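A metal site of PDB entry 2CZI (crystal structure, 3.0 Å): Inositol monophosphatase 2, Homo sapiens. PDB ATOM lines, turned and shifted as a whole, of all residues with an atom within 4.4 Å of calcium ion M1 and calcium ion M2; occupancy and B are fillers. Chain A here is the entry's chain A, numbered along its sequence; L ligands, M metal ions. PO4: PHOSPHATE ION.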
ATOM      1  N   ASP A  69      31.493   7.878   9.945  1.00  0.00           N
ATOM      2  CA  ASP A  69      31.241   6.749   9.041  1.00  0.00           C
ATOM      3  C   ASP A  69      31.536   5.452   9.764  1.00  0.00           C
ATOM      4  O   ASP A  69      30.786   4.493   9.654  1.00  0.00           O
ATOM      5  CB  ASP A  69      32.110   6.872   7.783  1.00  0.00           C
ATOM      6  CG  ASP A  69      31.657   5.931   6.680  1.00  0.00           C
ATOM      7  OD1 ASP A  69      31.734   6.266   5.487  1.00  0.00           O
ATOM      8  OD2 ASP A  69      31.206   4.823   7.021  1.00  0.00           O
ATOM      9  N   GLU A  92      30.803  -0.187   2.873  1.00  0.00           N
ATOM     10  CA  GLU A  92      32.002   0.456   2.347  1.00  0.00           C
ATOM     11  C   GLU A  92      33.326   0.071   3.014  1.00  0.00           C
ATOM     12  O   GLU A  92      34.364  -0.034   2.344  1.00  0.00           O
ATOM     13  CB  GLU A  92      31.848   1.974   2.334  1.00  0.00           C
ATOM     14  CG  GLU A  92      31.624   2.443   0.916  1.00  0.00           C
ATOM     15  CD  GLU A  92      31.817   3.923   0.810  1.00  0.00           C
ATOM     16  OE1 GLU A  92      30.953   4.634   1.341  1.00  0.00           O
ATOM     17  OE2 GLU A  92      32.846   4.384   0.232  1.00  0.00           O
ATOM     18  N   ASP A 112      25.536   1.066   3.271  1.00  0.00           N
ATOM     19  CA  ASP A 112      26.418   2.166   2.938  1.00  0.00           C
ATOM     20  C   ASP A 112      26.132   3.134   4.103  1.00  0.00           C
ATOM     21  O   ASP A 112      25.274   4.001   4.020  1.00  0.00           O
ATOM     22  CB  ASP A 112      26.028   2.772   1.597  1.00  0.00           C
ATOM     23  CG  ASP A 112      27.036   3.768   1.112  1.00  0.00           C
ATOM     24  OD1 ASP A 112      26.912   4.243  -0.024  1.00  0.00           O
ATOM     25  OD2 ASP A 112      27.968   4.064   1.886  1.00  0.00           O
ATOM     26  N   ILE A 114      27.220   5.765   5.177  1.00  0.00           N
ATOM     27  CA  ILE A 114      27.091   7.166   4.843  1.00  0.00           C
ATOM     28  C   ILE A 114      27.331   7.378   3.358  1.00  0.00           C
ATOM     29  O   ILE A 114      28.465   7.299   2.947  1.00  0.00           O
ATOM     30  CB  ILE A 114      28.138   8.032   5.598  1.00  0.00           C
ATOM     31  CG1 ILE A 114      27.897   7.934   7.103  1.00  0.00           C
ATOM     32  CG2 ILE A 114      28.094   9.499   5.102  1.00  0.00           C
ATOM     33  CD1 ILE A 114      28.693   8.917   7.932  1.00  0.00           C
ATOM     34  N   ASP A 115      26.286   7.641   2.581  1.00  0.00           N
ATOM     35  CA  ASP A 115      26.424   7.879   1.134  1.00  0.00           C
ATOM     36  C   ASP A 115      26.545   9.384   0.925  1.00  0.00           C
ATOM     37  O   ASP A 115      25.573  10.123   1.111  1.00  0.00           O
ATOM     38  CB  ASP A 115      25.188   7.363   0.382  1.00  0.00           C
ATOM     39  CG  ASP A 115      25.270   7.625  -1.117  1.00  0.00           C
ATOM     40  OD1 ASP A 115      24.301   8.168  -1.691  1.00  0.00           O
ATOM     41  OD2 ASP A 115      26.287   7.268  -1.739  1.00  0.00           O
ATOM     42  N   TRP A 241      26.468  -1.627  -2.724  1.00  0.00           N
ATOM     43  CA  TRP A 241      25.797  -1.117  -1.541  1.00  0.00           C
ATOM     44  C   TRP A 241      25.069   0.195  -1.780  1.00  0.00           C
ATOM     45  O   TRP A 241      24.396   0.693  -0.895  1.00  0.00           O
ATOM     46  CB  TRP A 241      26.785  -0.947  -0.394  1.00  0.00           C
ATOM     47  CG  TRP A 241      27.997  -0.184  -0.773  1.00  0.00           C
ATOM     48  CD1 TRP A 241      28.081   1.129  -1.073  1.00  0.00           C
ATOM     49  CD2 TRP A 241      29.322  -0.711  -0.886  1.00  0.00           C
ATOM     50  NE1 TRP A 241      29.377   1.472  -1.371  1.00  0.00           N
ATOM     51  CE2 TRP A 241      30.163   0.355  -1.267  1.00  0.00           C
ATOM     52  CE3 TRP A 241      29.882  -1.988  -0.712  1.00  0.00           C
ATOM     53  CZ2 TRP A 241      31.531   0.189  -1.477  1.00  0.00           C
ATOM     54  CZ3 TRP A 241      31.242  -2.151  -0.917  1.00  0.00           C
ATOM     55  CH2 TRP A 241      32.057  -1.057  -1.299  1.00  0.00           C
ATOM     56  N   ASP A 242      25.202   0.749  -2.979  1.00  0.00           N
ATOM     57  CA  ASP A 242      24.530   2.000  -3.290  1.00  0.00           C
ATOM     58  C   ASP A 242      23.150   1.724  -3.828  1.00  0.00           C
ATOM     59  O   ASP A 242      22.149   2.236  -3.322  1.00  0.00           O
ATOM     60  CB  ASP A 242      25.298   2.783  -4.343  1.00  0.00           C
ATOM     61  CG  ASP A 242      26.616   3.318  -3.832  1.00  0.00           C
ATOM     62  OD1 ASP A 242      26.626   3.872  -2.715  1.00  0.00           O
ATOM     63  OD2 ASP A 242      27.627   3.196  -4.560  1.00  0.00           O
HETATM   64  P   PO4 L   1      30.639   7.825  -0.342  1.00  0.00           P
HETATM   65  O1  PO4 L   1      31.719   7.291  -1.236  1.00  0.00           O
HETATM   66  O2  PO4 L   1      29.494   6.867  -0.303  1.00  0.00           O
HETATM   67  O3  PO4 L   1      31.156   8.001   1.055  1.00  0.00           O
HETATM   68  O4  PO4 L   1      30.147   9.156  -0.852  1.00  0.00           O
HETATM   69 CA    CA M   1      28.343   5.458  -1.763  1.00  0.00          CA
HETATM   70 CA    CA M   2      29.515   5.882   1.810  1.00  0.00          CA
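Calcium ion M2 is bound by OE1 of Glu 92 (2.0 Å), O of Ile 114 (2.1 Å), O2 of the ligand (2.3 Å), OD2 of Asp 112 (2.4 Å) and O3 of the ligand (2.8 Å).
Calcium ion M2 has five donor atoms within binding distance.
Of the 7 residues printed, 4 come within 4 Å of calcium ion M2.
Calcium ion M1 is bound by an oxygen (O2) of the ligand, the side-chain carboxylate (OD1) of Asp 242, the side-chain carboxylate (OD1) of Asp 112 and the side-chain carboxylate (OD2) of Asp 115.
Within 4 Å of calcium ion M1: Asp 112, Asp 115 and Asp 242.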
